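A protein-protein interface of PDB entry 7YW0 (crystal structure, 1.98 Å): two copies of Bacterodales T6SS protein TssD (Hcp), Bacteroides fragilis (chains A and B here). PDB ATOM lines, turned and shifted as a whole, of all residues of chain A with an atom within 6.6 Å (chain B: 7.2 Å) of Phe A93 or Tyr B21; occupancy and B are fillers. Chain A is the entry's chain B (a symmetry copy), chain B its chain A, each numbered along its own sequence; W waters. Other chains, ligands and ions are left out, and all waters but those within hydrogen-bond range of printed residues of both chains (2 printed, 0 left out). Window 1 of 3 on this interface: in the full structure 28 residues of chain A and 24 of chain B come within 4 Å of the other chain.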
ATOM      1  N   THR A  52     -19.481 -32.661 -12.870  1.00  0.00           N
ATOM      2  CA  THR A  52     -19.613 -31.774 -11.715  1.00  0.00           C
ATOM      3  C   THR A  52     -18.744 -30.548 -11.894  1.00  0.00           C
ATOM      4  O   THR A  52     -18.445 -29.824 -10.923  1.00  0.00           O
ATOM      5  CB  THR A  52     -19.358 -32.449 -10.355  1.00  0.00           C
ATOM      6  OG1 THR A  52     -18.063 -33.032 -10.407  1.00  0.00           O
ATOM      7  CG2 THR A  52     -20.391 -33.495  -9.978  1.00  0.00           C
ATOM      8  N   ILE A  54     -19.330 -27.516 -13.194  1.00  0.00           N
ATOM      9  CA  ILE A  54     -19.854 -26.207 -12.814  1.00  0.00           C
ATOM     10  C   ILE A  54     -19.715 -26.034 -11.308  1.00  0.00           C
ATOM     11  O   ILE A  54     -19.151 -25.050 -10.828  1.00  0.00           O
ATOM     12  CB  ILE A  54     -21.277 -25.979 -13.362  1.00  0.00           C
ATOM     13  CG1 ILE A  54     -21.233 -25.997 -14.899  1.00  0.00           C
ATOM     14  CG2 ILE A  54     -21.814 -24.643 -12.853  1.00  0.00           C
ATOM     15  CD1 ILE A  54     -22.557 -26.288 -15.574  1.00  0.00           C
ATOM     16  N   LEU A  55     -20.227 -27.023 -10.547  1.00  0.00           N
ATOM     17  CA  LEU A  55     -20.135 -26.906  -9.106  1.00  0.00           C
ATOM     18  C   LEU A  55     -18.670 -26.835  -8.649  1.00  0.00           C
ATOM     19  O   LEU A  55     -18.315 -26.069  -7.721  1.00  0.00           O
ATOM     20  CB  LEU A  55     -20.876 -28.088  -8.466  1.00  0.00           C
ATOM     21  CG  LEU A  55     -21.013 -28.017  -6.945  1.00  0.00           C
ATOM     22  CD1 LEU A  55     -21.729 -26.733  -6.518  1.00  0.00           C
ATOM     23  CD2 LEU A  55     -21.739 -29.262  -6.412  1.00  0.00           C
ATOM     24  N   GLU A  56     -17.808 -27.667  -9.250  1.00  0.00           N
ATOM     25  CA  GLU A  56     -16.421 -27.627  -8.792  1.00  0.00           C
ATOM     26  C   GLU A  56     -15.900 -26.215  -8.981  1.00  0.00           C
ATOM     27  O   GLU A  56     -15.157 -25.684  -8.151  1.00  0.00           O
ATOM     28  CB  GLU A  56     -15.493 -28.582  -9.540  1.00  0.00           C
ATOM     29  CG  GLU A  56     -15.611 -30.014  -9.081  1.00  0.00           C
ATOM     30  CD  GLU A  56     -15.351 -30.930 -10.252  1.00  0.00           C
ATOM     31  OE1 GLU A  56     -14.719 -30.468 -11.209  1.00  0.00           O
ATOM     32  OE2 GLU A  56     -15.857 -32.058 -10.260  1.00  0.00           O
ATOM     33  N   MET A  58     -17.488 -23.522  -8.735  1.00  0.00           N
ATOM     34  CA  MET A  58     -17.910 -22.671  -7.638  1.00  0.00           C
ATOM     35  C   MET A  58     -17.189 -23.055  -6.340  1.00  0.00           C
ATOM     36  O   MET A  58     -16.758 -22.183  -5.589  1.00  0.00           O
ATOM     37  CB  MET A  58     -19.430 -22.775  -7.413  1.00  0.00           C
ATOM     38  CG  MET A  58     -19.960 -21.780  -6.403  1.00  0.00           C
ATOM     39  SD  MET A  58     -21.688 -22.105  -6.016  1.00  0.00           S
ATOM     40  CE  MET A  58     -22.208 -20.587  -5.229  1.00  0.00           C
ATOM     41  N   ILE A  90     -19.196 -17.763  -9.978  1.00  0.00           N
ATOM     42  CA  ILE A  90     -20.517 -18.356  -9.873  1.00  0.00           C
ATOM     43  C   ILE A  90     -21.043 -18.042  -8.481  1.00  0.00           C
ATOM     44  O   ILE A  90     -20.474 -18.488  -7.495  1.00  0.00           O
ATOM     45  CB  ILE A  90     -20.451 -19.871 -10.110  1.00  0.00           C
ATOM     46  CG1 ILE A  90     -20.142 -20.250 -11.557  1.00  0.00           C
ATOM     47  CG2 ILE A  90     -21.694 -20.564  -9.558  1.00  0.00           C
ATOM     48  CD1 ILE A  90     -19.842 -21.752 -11.690  1.00  0.00           C
ATOM     49  N   THR A  91     -22.155 -17.314  -8.409  1.00  0.00           N
ATOM     50  CA  THR A  91     -22.583 -16.815  -7.120  1.00  0.00           C
ATOM     51  C   THR A  91     -23.898 -17.459  -6.701  1.00  0.00           C
ATOM     52  O   THR A  91     -24.423 -17.183  -5.623  1.00  0.00           O
ATOM     53  CB  THR A  91     -22.676 -15.283  -7.138  1.00  0.00           C
ATOM     54  OG1 THR A  91     -23.649 -14.915  -8.106  1.00  0.00           O
ATOM     55  CG2 THR A  91     -21.359 -14.646  -7.503  1.00  0.00           C
ATOM     56  N   GLU A  92     -24.411 -18.366  -7.529  1.00  0.00           N
ATOM     57  CA  GLU A  92     -25.609 -19.057  -7.137  1.00  0.00           C
ATOM     58  C   GLU A  92     -25.660 -20.317  -7.977  1.00  0.00           C
ATOM     59  O   GLU A  92     -25.376 -20.244  -9.162  1.00  0.00           O
ATOM     60  CB  GLU A  92     -26.811 -18.134  -7.363  1.00  0.00           C
ATOM     61  CG  GLU A  92     -28.102 -18.691  -6.800  1.00  0.00           C
ATOM     62  CD  GLU A  92     -29.301 -17.887  -7.283  1.00  0.00           C
ATOM     63  OE1 GLU A  92     -30.232 -18.506  -7.855  1.00  0.00           O
ATOM     64  OE2 GLU A  92     -29.271 -16.641  -7.139  1.00  0.00           O
ATOM     65  N   PHE A  93     -25.908 -21.448  -7.313  1.00  0.00           N
ATOM     66  CA  PHE A  93     -25.994 -22.760  -7.925  1.00  0.00           C
ATOM     67  C   PHE A  93     -27.138 -23.510  -7.255  1.00  0.00           C
ATOM     68  O   PHE A  93     -27.279 -23.442  -6.039  1.00  0.00           O
ATOM     69  CB  PHE A  93     -24.666 -23.510  -7.738  1.00  0.00           C
ATOM     70  CG  PHE A  93     -24.620 -24.911  -8.277  1.00  0.00           C
ATOM     71  CD1 PHE A  93     -25.205 -25.960  -7.579  1.00  0.00           C
ATOM     72  CD2 PHE A  93     -23.918 -25.195  -9.438  1.00  0.00           C
ATOM     73  CE1 PHE A  93     -25.168 -27.243  -8.088  1.00  0.00           C
ATOM     74  CE2 PHE A  93     -23.874 -26.488  -9.935  1.00  0.00           C
ATOM     75  CZ  PHE A  93     -24.473 -27.506  -9.239  1.00  0.00           C
ATOM     76  N   THR A  94     -27.901 -24.245  -8.076  1.00  0.00           N
ATOM     77  CA  THR A  94     -28.908 -25.171  -7.639  1.00  0.00           C
ATOM     78  C   THR A  94     -28.914 -26.334  -8.622  1.00  0.00           C
ATOM     79  O   THR A  94     -28.844 -26.127  -9.831  1.00  0.00           O
ATOM     80  CB  THR A  94     -30.276 -24.486  -7.759  1.00  0.00           C
ATOM     81  OG1 THR A  94     -30.241 -23.356  -6.884  1.00  0.00           O
ATOM     82  CG2 THR A  94     -31.435 -25.386  -7.407  1.00  0.00           C
ATOM     83  N   GLU A  95     -28.992 -27.564  -8.119  1.00  0.00           N
ATOM     84  CA  GLU A  95     -29.199 -28.669  -9.047  1.00  0.00           C
ATOM     85  C   GLU A  95     -30.483 -29.348  -8.611  1.00  0.00           C
ATOM     86  O   GLU A  95     -30.702 -29.486  -7.400  1.00  0.00           O
ATOM     87  CB  GLU A  95     -28.046 -29.690  -8.915  1.00  0.00           C
ATOM     88  CG  GLU A  95     -28.111 -30.878  -9.890  1.00  0.00           C
ATOM     89  CD  GLU A  95     -26.757 -31.541 -10.256  1.00  0.00           C
ATOM     90  OE1 GLU A  95     -25.803 -31.505  -9.424  1.00  0.00           O
ATOM     91  OE2 GLU A  95     -26.640 -32.133 -11.377  1.00  0.00           O
ATOM     92  N   ASN A  96     -31.297 -29.802  -9.580  1.00  0.00           N
ATOM     93  CA  ASN A  96     -32.584 -30.391  -9.222  1.00  0.00           C
ATOM     94  C   ASN A  96     -32.788 -31.669 -10.032  1.00  0.00           C
ATOM     95  O   ASN A  96     -32.397 -31.702 -11.187  1.00  0.00           O
ATOM     96  CB  ASN A  96     -33.738 -29.395  -9.425  1.00  0.00           C
ATOM     97  CG  ASN A  96     -35.098 -30.077  -9.449  1.00  0.00           C
ATOM     98  OD1 ASN A  96     -35.684 -30.390  -8.405  1.00  0.00           O
ATOM     99  ND2 ASN A  96     -35.572 -30.366 -10.651  1.00  0.00           N
ATOM    100  N   ILE A  97     -33.319 -32.718  -9.387  1.00  0.00           N
ATOM    101  CA  ILE A  97     -33.700 -33.973 -10.023  1.00  0.00           C
ATOM    102  C   ILE A  97     -35.194 -34.137  -9.793  1.00  0.00           C
ATOM    103  O   ILE A  97     -35.676 -33.840  -8.700  1.00  0.00           O
ATOM    104  CB  ILE A  97     -32.923 -35.135  -9.363  1.00  0.00           C
ATOM    105  CG1 ILE A  97     -31.423 -34.847  -9.275  1.00  0.00           C
ATOM    106  CG2 ILE A  97     -33.202 -36.469 -10.047  1.00  0.00           C
ATOM    107  CD1 ILE A  97     -31.007 -33.873  -8.186  1.00  0.00           C
ATOM    108  N   MET A 105     -33.193 -33.701 -14.934  1.00  0.00           N
ATOM    109  CA  MET A 105     -32.097 -33.351 -14.049  1.00  0.00           C
ATOM    110  C   MET A 105     -31.337 -32.162 -14.621  1.00  0.00           C
ATOM    111  O   MET A 105     -30.835 -32.244 -15.738  1.00  0.00           O
ATOM    112  CB  MET A 105     -31.139 -34.535 -13.891  1.00  0.00           C
ATOM    113  CG  MET A 105     -30.163 -34.317 -12.752  1.00  0.00           C
ATOM    114  SD  MET A 105     -29.388 -35.809 -12.077  1.00  0.00           S
ATOM    115  CE  MET A 105     -28.317 -35.114 -10.820  1.00  0.00           C
ATOM    116  N   ILE A 107     -29.166 -28.082 -13.861  1.00  0.00           N
ATOM    117  CA  ILE A 107     -28.469 -27.111 -13.028  1.00  0.00           C
ATOM    118  C   ILE A 107     -28.939 -25.699 -13.389  1.00  0.00           C
ATOM    119  O   ILE A 107     -29.001 -25.344 -14.560  1.00  0.00           O
ATOM    120  CB  ILE A 107     -26.955 -27.296 -13.256  1.00  0.00           C
ATOM    121  CG1 ILE A 107     -26.470 -28.592 -12.584  1.00  0.00           C
ATOM    122  CG2 ILE A 107     -26.184 -26.097 -12.716  1.00  0.00           C
ATOM    123  CD1 ILE A 107     -25.063 -29.009 -13.021  1.00  0.00           C
ATOM    124  N   THR A 108     -29.183 -24.859 -12.376  1.00  0.00           N
ATOM    125  CA  THR A 108     -29.420 -23.457 -12.635  1.00  0.00           C
ATOM    126  C   THR A 108     -28.359 -22.712 -11.841  1.00  0.00           C
ATOM    127  O   THR A 108     -28.229 -22.982 -10.666  1.00  0.00           O
ATOM    128  CB  THR A 108     -30.827 -23.064 -12.172  1.00  0.00           C
ATOM    129  OG1 THR A 108     -31.694 -23.933 -12.901  1.00  0.00           O
ATOM    130  CG2 THR A 108     -31.168 -21.625 -12.485  1.00  0.00           C
ATOM    131  N   PHE A 109     -27.562 -21.871 -12.508  1.00  0.00           N
ATOM    132  CA  PHE A 109     -26.524 -21.131 -11.821  1.00  0.00           C
ATOM    133  C   PHE A 109     -26.448 -19.715 -12.376  1.00  0.00           C
ATOM    134  O   PHE A 109     -26.877 -19.474 -13.496  1.00  0.00           O
ATOM    135  CB  PHE A 109     -25.212 -21.919 -11.931  1.00  0.00           C
ATOM    136  CG  PHE A 109     -24.479 -21.901 -13.250  1.00  0.00           C
ATOM    137  CD1 PHE A 109     -24.861 -22.720 -14.297  1.00  0.00           C
ATOM    138  CD2 PHE A 109     -23.368 -21.091 -13.440  1.00  0.00           C
ATOM    139  CE1 PHE A 109     -24.178 -22.699 -15.503  1.00  0.00           C
ATOM    140  CE2 PHE A 109     -22.665 -21.097 -14.638  1.00  0.00           C
ATOM    141  CZ  PHE A 109     -23.067 -21.908 -15.678  1.00  0.00           C
ATOM    142  N   VAL A 110     -25.888 -18.796 -11.575  1.00  0.00           N
ATOM    143  CA  VAL A 110     -25.788 -17.381 -11.895  1.00  0.00           C
ATOM    144  C   VAL A 110     -24.301 -17.019 -11.899  1.00  0.00           C
ATOM    145  O   VAL A 110     -23.576 -17.453 -11.015  1.00  0.00           O
ATOM    146  CB  VAL A 110     -26.553 -16.525 -10.867  1.00  0.00           C
ATOM    147  CG1 VAL A 110     -26.245 -15.043 -10.993  1.00  0.00           C
ATOM    148  CG2 VAL A 110     -28.053 -16.766 -10.888  1.00  0.00           C
ATOM    149  N   CYS B  19     -35.178 -34.229  -5.703  1.00  0.00           N
ATOM    150  CA  CYS B  19     -34.103 -33.808  -4.822  1.00  0.00           C
ATOM    151  C   CYS B  19     -33.546 -32.473  -5.308  1.00  0.00           C
ATOM    152  O   CYS B  19     -33.359 -32.297  -6.513  1.00  0.00           O
ATOM    153  CB  CYS B  19     -32.982 -34.854  -4.897  1.00  0.00           C
ATOM    154  SG  CYS B  19     -31.516 -34.353  -3.952  1.00  0.00           S
ATOM    155  N   THR B  20     -33.227 -31.534  -4.389  1.00  0.00           N
ATOM    156  CA  THR B  20     -32.593 -30.303  -4.809  1.00  0.00           C
ATOM    157  C   THR B  20     -31.647 -29.837  -3.712  1.00  0.00           C
ATOM    158  O   THR B  20     -31.920 -30.050  -2.547  1.00  0.00           O
ATOM    159  CB  THR B  20     -33.648 -29.245  -5.213  1.00  0.00           C
ATOM    160  OG1 THR B  20     -32.989 -28.073  -5.676  1.00  0.00           O
ATOM    161  CG2 THR B  20     -34.497 -28.717  -4.087  1.00  0.00           C
ATOM    162  N   TYR B  21     -30.524 -29.253  -4.107  1.00  0.00           N
ATOM    163  CA  TYR B  21     -29.575 -28.652  -3.177  1.00  0.00           C
ATOM    164  C   TYR B  21     -29.110 -27.369  -3.820  1.00  0.00           C
ATOM    165  O   TYR B  21     -29.183 -27.228  -5.043  1.00  0.00           O
ATOM    166  CB  TYR B  21     -28.421 -29.589  -2.778  1.00  0.00           C
ATOM    167  CG  TYR B  21     -27.474 -29.929  -3.890  1.00  0.00           C
ATOM    168  CD1 TYR B  21     -27.803 -30.913  -4.802  1.00  0.00           C
ATOM    169  CD2 TYR B  21     -26.295 -29.221  -4.068  1.00  0.00           C
ATOM    170  CE1 TYR B  21     -26.983 -31.174  -5.884  1.00  0.00           C
ATOM    171  CE2 TYR B  21     -25.436 -29.513  -5.116  1.00  0.00           C
ATOM    172  CZ  TYR B  21     -25.795 -30.484  -6.034  1.00  0.00           C
ATOM    173  OH  TYR B  21     -24.993 -30.742  -7.119  1.00  0.00           O
ATOM    174  N   SER B  22     -28.690 -26.427  -2.989  1.00  0.00           N
ATOM    175  CA  SER B  22     -28.402 -25.127  -3.547  1.00  0.00           C
ATOM    176  C   SER B  22     -27.308 -24.499  -2.679  1.00  0.00           C
ATOM    177  O   SER B  22     -27.148 -24.907  -1.523  1.00  0.00           O
ATOM    178  CB  SER B  22     -29.701 -24.310  -3.590  1.00  0.00           C
ATOM    179  OG  SER B  22     -29.692 -23.268  -2.615  1.00  0.00           O
ATOM    180  N   LEU B  23     -26.511 -23.626  -3.302  1.00  0.00           N
ATOM    181  CA  LEU B  23     -25.424 -22.891  -2.674  1.00  0.00           C
ATOM    182  C   LEU B  23     -25.460 -21.486  -3.262  1.00  0.00           C
ATOM    183  O   LEU B  23     -25.937 -21.291  -4.381  1.00  0.00           O
ATOM    184  CB  LEU B  23     -24.101 -23.578  -3.040  1.00  0.00           C
ATOM    185  CG  LEU B  23     -23.950 -25.003  -2.506  1.00  0.00           C
ATOM    186  CD1 LEU B  23     -22.959 -25.814  -3.300  1.00  0.00           C
ATOM    187  CD2 LEU B  23     -23.534 -24.985  -1.053  1.00  0.00           C
ATOM    188  N   LYS B  24     -24.930 -20.520  -2.506  1.00  0.00           N
ATOM    189  CA  LYS B  24     -25.069 -19.109  -2.842  1.00  0.00           C
ATOM    190  C   LYS B  24     -23.912 -18.322  -2.228  1.00  0.00           C
ATOM    191  O   LYS B  24     -23.344 -18.762  -1.224  1.00  0.00           O
ATOM    192  CB  LYS B  24     -26.427 -18.655  -2.309  1.00  0.00           C
ATOM    193  CG  LYS B  24     -26.800 -17.197  -2.502  1.00  0.00           C
ATOM    194  CD  LYS B  24     -28.279 -17.021  -2.252  1.00  0.00           C
ATOM    195  CE  LYS B  24     -28.717 -15.580  -2.126  1.00  0.00           C
ATOM    196  NZ  LYS B  24     -28.678 -14.864  -3.423  1.00  0.00           N
ATOM    197  N   ARG B  25     -23.536 -17.202  -2.873  1.00  0.00           N
ATOM    198  CA  ARG B  25     -22.647 -16.195  -2.304  1.00  0.00           C
ATOM    199  C   ARG B  25     -23.266 -14.818  -2.515  1.00  0.00           C
ATOM    200  O   ARG B  25     -23.832 -14.564  -3.556  1.00  0.00           O
ATOM    201  CB  ARG B  25     -21.338 -16.147  -3.097  1.00  0.00           C
ATOM    202  CG  ARG B  25     -20.534 -17.431  -2.972  1.00  0.00           C
ATOM    203  CD  ARG B  25     -19.310 -17.446  -3.845  1.00  0.00           C
ATOM    204  NE  ARG B  25     -18.449 -16.369  -3.395  1.00  0.00           N
ATOM    205  CZ  ARG B  25     -17.242 -16.164  -3.904  1.00  0.00           C
ATOM    206  NH1 ARG B  25     -16.790 -16.972  -4.852  1.00  0.00           N
ATOM    207  NH2 ARG B  25     -16.500 -15.159  -3.467  1.00  0.00           N
ATOM    208  N   GLY B  40     -26.254 -25.223   1.000  1.00  0.00           N
ATOM    209  CA  GLY B  40     -25.886 -26.632   0.936  1.00  0.00           C
ATOM    210  C   GLY B  40     -26.860 -27.552   1.675  1.00  0.00           C
ATOM    211  O   GLY B  40     -26.544 -28.713   1.914  1.00  0.00           O
ATOM    212  N   GLN B  41     -28.038 -27.033   2.045  1.00  0.00           N
ATOM    213  CA  GLN B  41     -29.124 -27.844   2.566  1.00  0.00           C
ATOM    214  C   GLN B  41     -29.608 -28.730   1.419  1.00  0.00           C
ATOM    215  O   GLN B  41     -29.592 -28.285   0.282  1.00  0.00           O
ATOM    216  CB  GLN B  41     -30.240 -26.898   3.037  1.00  0.00           C
ATOM    217  CG  GLN B  41     -29.962 -26.213   4.376  1.00  0.00           C
ATOM    218  CD  GLN B  41     -31.239 -25.608   4.918  1.00  0.00           C
ATOM    219  OE1 GLN B  41     -31.954 -24.882   4.230  1.00  0.00           O
ATOM    220  NE2 GLN B  41     -31.562 -25.908   6.165  1.00  0.00           N
ATOM    221  N   ILE B  42     -29.964 -29.988   1.697  1.00  0.00           N
ATOM    222  CA  ILE B  42     -30.498 -30.860   0.651  1.00  0.00           C
ATOM    223  C   ILE B  42     -31.998 -31.079   0.883  1.00  0.00           C
ATOM    224  O   ILE B  42     -32.389 -31.471   1.979  1.00  0.00           O
ATOM    225  CB  ILE B  42     -29.746 -32.185   0.713  1.00  0.00           C
ATOM    226  CG1 ILE B  42     -28.236 -31.974   0.600  1.00  0.00           C
ATOM    227  CG2 ILE B  42     -30.301 -33.184  -0.302  1.00  0.00           C
ATOM    228  CD1 ILE B  42     -27.378 -33.194   1.073  1.00  0.00           C
ATOM    229  N   ARG B  43     -32.840 -30.928  -0.158  1.00  0.00           N
ATOM    230  CA  ARG B  43     -34.256 -31.088   0.092  1.00  0.00           C
ATOM    231  C   ARG B  43     -34.723 -32.361  -0.598  1.00  0.00           C
ATOM    232  O   ARG B  43     -34.502 -32.506  -1.791  1.00  0.00           O
ATOM    233  CB  ARG B  43     -35.015 -29.844  -0.404  1.00  0.00           C
ATOM    234  CG  ARG B  43     -36.536 -29.963  -0.330  1.00  0.00           C
ATOM    235  CD  ARG B  43     -37.288 -28.766  -0.920  1.00  0.00           C
ATOM    236  NE  ARG B  43     -38.580 -29.106  -1.515  1.00  0.00           N
ATOM    237  CZ  ARG B  43     -39.772 -28.673  -1.078  1.00  0.00           C
ATOM    238  NH1 ARG B  43     -39.848 -27.872  -0.027  1.00  0.00           N
ATOM    239  NH2 ARG B  43     -40.887 -29.044  -1.687  1.00  0.00           N
ATOM    240  N   PHE B  71     -27.676 -41.310  -8.380  1.00  0.00           N
ATOM    241  CA  PHE B  71     -28.447 -41.001  -9.576  1.00  0.00           C
ATOM    242  C   PHE B  71     -28.029 -41.925 -10.713  1.00  0.00           C
ATOM    243  O   PHE B  71     -26.843 -42.098 -10.964  1.00  0.00           O
ATOM    244  CB  PHE B  71     -28.195 -39.561  -9.995  1.00  0.00           C
ATOM    245  CG  PHE B  71     -28.418 -38.556  -8.900  1.00  0.00           C
ATOM    246  CD1 PHE B  71     -29.686 -38.077  -8.643  1.00  0.00           C
ATOM    247  CD2 PHE B  71     -27.366 -38.087  -8.134  1.00  0.00           C
ATOM    248  CE1 PHE B  71     -29.900 -37.127  -7.655  1.00  0.00           C
ATOM    249  CE2 PHE B  71     -27.583 -37.124  -7.160  1.00  0.00           C
ATOM    250  CZ  PHE B  71     -28.848 -36.661  -6.911  1.00  0.00           C
ATOM    251  N   LYS B  81     -23.737 -40.330 -10.961  1.00  0.00           N
ATOM    252  CA  LYS B  81     -23.022 -39.569  -9.947  1.00  0.00           C
ATOM    253  C   LYS B  81     -23.763 -39.708  -8.626  1.00  0.00           C
ATOM    254  O   LYS B  81     -24.852 -40.279  -8.586  1.00  0.00           O
ATOM    255  CB  LYS B  81     -22.866 -38.093 -10.326  1.00  0.00           C
ATOM    256  CG  LYS B  81     -24.134 -37.240 -10.381  1.00  0.00           C
ATOM    257  CD  LYS B  81     -23.739 -35.868 -10.915  1.00  0.00           C
ATOM    258  CE  LYS B  81     -24.849 -34.896 -11.235  1.00  0.00           C
ATOM    259  NZ  LYS B  81     -24.305 -33.566 -11.648  1.00  0.00           N
ATOM    260  N   LEU B  83     -24.496 -37.866  -4.685  1.00  0.00           N
ATOM    261  CA  LEU B  83     -24.470 -36.787  -3.710  1.00  0.00           C
ATOM    262  C   LEU B  83     -24.444 -37.474  -2.349  1.00  0.00           C
ATOM    263  O   LEU B  83     -25.270 -38.361  -2.071  1.00  0.00           O
ATOM    264  CB  LEU B  83     -25.717 -35.903  -3.882  1.00  0.00           C
ATOM    265  CG  LEU B  83     -26.017 -34.868  -2.789  1.00  0.00           C
ATOM    266  CD1 LEU B  83     -24.934 -33.819  -2.736  1.00  0.00           C
ATOM    267  CD2 LEU B  83     -27.370 -34.177  -3.021  1.00  0.00           C
ATOM    268  N   ILE B 116     -21.088 -31.664   2.190  1.00  0.00           N
ATOM    269  CA  ILE B 116     -21.744 -32.353   1.090  1.00  0.00           C
ATOM    270  C   ILE B 116     -20.704 -32.547   0.007  1.00  0.00           C
ATOM    271  O   ILE B 116     -19.785 -31.731  -0.147  1.00  0.00           O
ATOM    272  CB  ILE B 116     -22.984 -31.584   0.557  1.00  0.00           C
ATOM    273  CG1 ILE B 116     -22.608 -30.250  -0.077  1.00  0.00           C
ATOM    274  CG2 ILE B 116     -24.017 -31.417   1.661  1.00  0.00           C
ATOM    275  CD1 ILE B 116     -23.798 -29.494  -0.734  1.00  0.00           C
ATOM    276  N   LYS B 117     -20.860 -33.644  -0.733  1.00  0.00           N
ATOM    277  CA  LYS B 117     -19.909 -33.979  -1.768  1.00  0.00           C
ATOM    278  C   LYS B 117     -20.693 -34.572  -2.934  1.00  0.00           C
ATOM    279  O   LYS B 117     -21.642 -35.292  -2.712  1.00  0.00           O
ATOM    280  CB  LYS B 117     -18.921 -35.038  -1.262  1.00  0.00           C
ATOM    281  CG  LYS B 117     -18.083 -34.612  -0.068  1.00  0.00           C
ATOM    282  CD  LYS B 117     -16.935 -35.566   0.209  1.00  0.00           C
ATOM    283  CE  LYS B 117     -16.180 -35.207   1.473  1.00  0.00           C
ATOM    284  NZ  LYS B 117     -15.417 -36.368   1.988  1.00  0.00           N
ATOM    285  N   ILE B 118     -20.252 -34.283  -4.152  1.00  0.00           N
ATOM    286  CA  ILE B 118     -20.804 -34.917  -5.344  1.00  0.00           C
ATOM    287  C   ILE B 118     -19.732 -34.799  -6.441  1.00  0.00           C
ATOM    288  O   ILE B 118     -19.002 -33.809  -6.469  1.00  0.00           O
ATOM    289  CB  ILE B 118     -22.166 -34.266  -5.707  1.00  0.00           C
ATOM    290  CG1 ILE B 118     -22.789 -34.847  -6.984  1.00  0.00           C
ATOM    291  CG2 ILE B 118     -21.999 -32.754  -5.817  1.00  0.00           C
ATOM    292  CD1 ILE B 118     -24.283 -34.537  -7.153  1.00  0.00           C
ATOM    293  N   ALA B 121     -16.773 -32.284  -6.477  1.00  0.00           N
ATOM    294  CA  ALA B 121     -17.015 -31.096  -5.657  1.00  0.00           C
ATOM    295  C   ALA B 121     -17.152 -31.479  -4.192  1.00  0.00           C
ATOM    296  O   ALA B 121     -17.732 -32.525  -3.889  1.00  0.00           O
ATOM    297  CB  ALA B 121     -18.277 -30.356  -6.109  1.00  0.00           C
HETATM  298  O   HOH W   1     -23.091 -31.037 -10.082  1.00  0.00           O
HETATM  299  O   HOH W   2     -17.799 -18.538  -6.729  1.00  0.00           O
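Of the printed residues of chain B, Thr A91 touches Lys B24 (3.4 Å) and Arg B25 (2.9 Å).
Phe A93 touches just these residues of chain B: Tyr B21 (3.6 Å), Ser B22 (3.2 Å) and Leu B23 (2.8 Å).
Of the printed residues of chain A, Thr B20 touches Thr A94, Glu A95 and Asn A96.
Of chain A, only Leu A55 (3.6 Å), Phe A93 (3.6 Å), Thr A94 (3.3 Å) and Glu A95 (2.6 Å) come within 4 Å of Tyr B21.
Of the printed residues of chain A, Arg B25 touches Ile A90 and Thr A91.
The nearest residue of chain A that does not touch Tyr B21 is Ile A97 (5.4 Å).
The nearest printed residue of chain B that does not touch Thr A52 is Ala B121 (4.2 Å).
No position is printed for both chains.
Of the 28 pairs that touch across the chains among the printed residues, none has its exchanged pair printed and touching as well.
Printed residues of chain A that touch a printed residue of chain B: Thr A52, Leu A55, Glu A56, Met A58, Ile A90, Thr A91, Glu A92, Phe A93, Thr A94, Glu A95, Asn A96, Ile A97 and Met A105.
Hydrophobic or aromatic side chains of chain A within 4 Å of the printed part of chain B: Leu A55, Met A58, Phe A93, Ile A97 and Met A105.
Along chain A the printed residues that touch a printed residue of chain B span positions 52 to 105.
OH of Tyr B21 is in hydrogen-bond range of OE1 of Glu A95, 2.6 Å away.
The backbone carbonyl oxygen (O) of Cys B19 sits at hydrogen-bond distance from the backbone NH (N) of Ile A97 (2.9 Å).
OG1 of Thr B20 lies within hydrogen-bond range of O of Glu A95 (3.2 Å).
N of Leu B23 sits at hydrogen-bond distance from O of Phe A93 (2.8 Å).
O of Thr A91 is in hydrogen-bond range of N of Arg B25, at 2.9 Å.
The side-chain carboxylate (OE2) of Glu A95 is in salt-bridge range of the side-chain amino group (NZ) of Lys B81 (2.8 Å).
The backbone NH of Phe B71 is in hydrogen-bond range of the backbone carbonyl oxygen of Lys B81, 3.0 Å away.
The backbone NH (N) of Val A110 lies within hydrogen-bond range of the backbone carbonyl oxygen (O) of Glu A92.
O of Ser B22 is in hydrogen-bond range of N of Gly B40 (2.7 Å).
The backbone carbonyl oxygen (O) of Thr A94 is in hydrogen-bond range of the backbone NH (N) of Thr A108.
The backbone carbonyl oxygen of Thr B20 lies within hydrogen-bond range of the backbone NH of Arg B43.
O of Val A110 sits at hydrogen-bond distance from N of Thr A91 (3.0 Å).
CD1 of Leu A55 touches CD1 of Leu B23, 3.6 Å away.
CD2 of Leu A55 touches CB of Ala B121 (3.6 Å).
O of Leu B23 touches CA of Glu A92, 3.6 Å away.
Thr A94 touches Thr B20 (CG2 to OG1, 3.6 Å).
O of Tyr B21 touches CA of Thr A94, 3.3 Å away.
O of Glu A95 touches O of Cys B19, 3.97 Å away.
Asn A96 touches Cys B19.
CB of Thr B20 touches OD1 of Asn A96 (3.96 Å).
CG1 of Ile A97 touches CE1 of Phe B71, at 3.2 Å.
Met A105 touches Phe B71.
Water W2 bridges NH1 of Arg B25 (2.6 Å) and O of Ile A90 (2.8 Å).
Water W1 bridges OE1 of Glu A95 (2.8 Å) and NZ of Lys B81 (3.2 Å).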
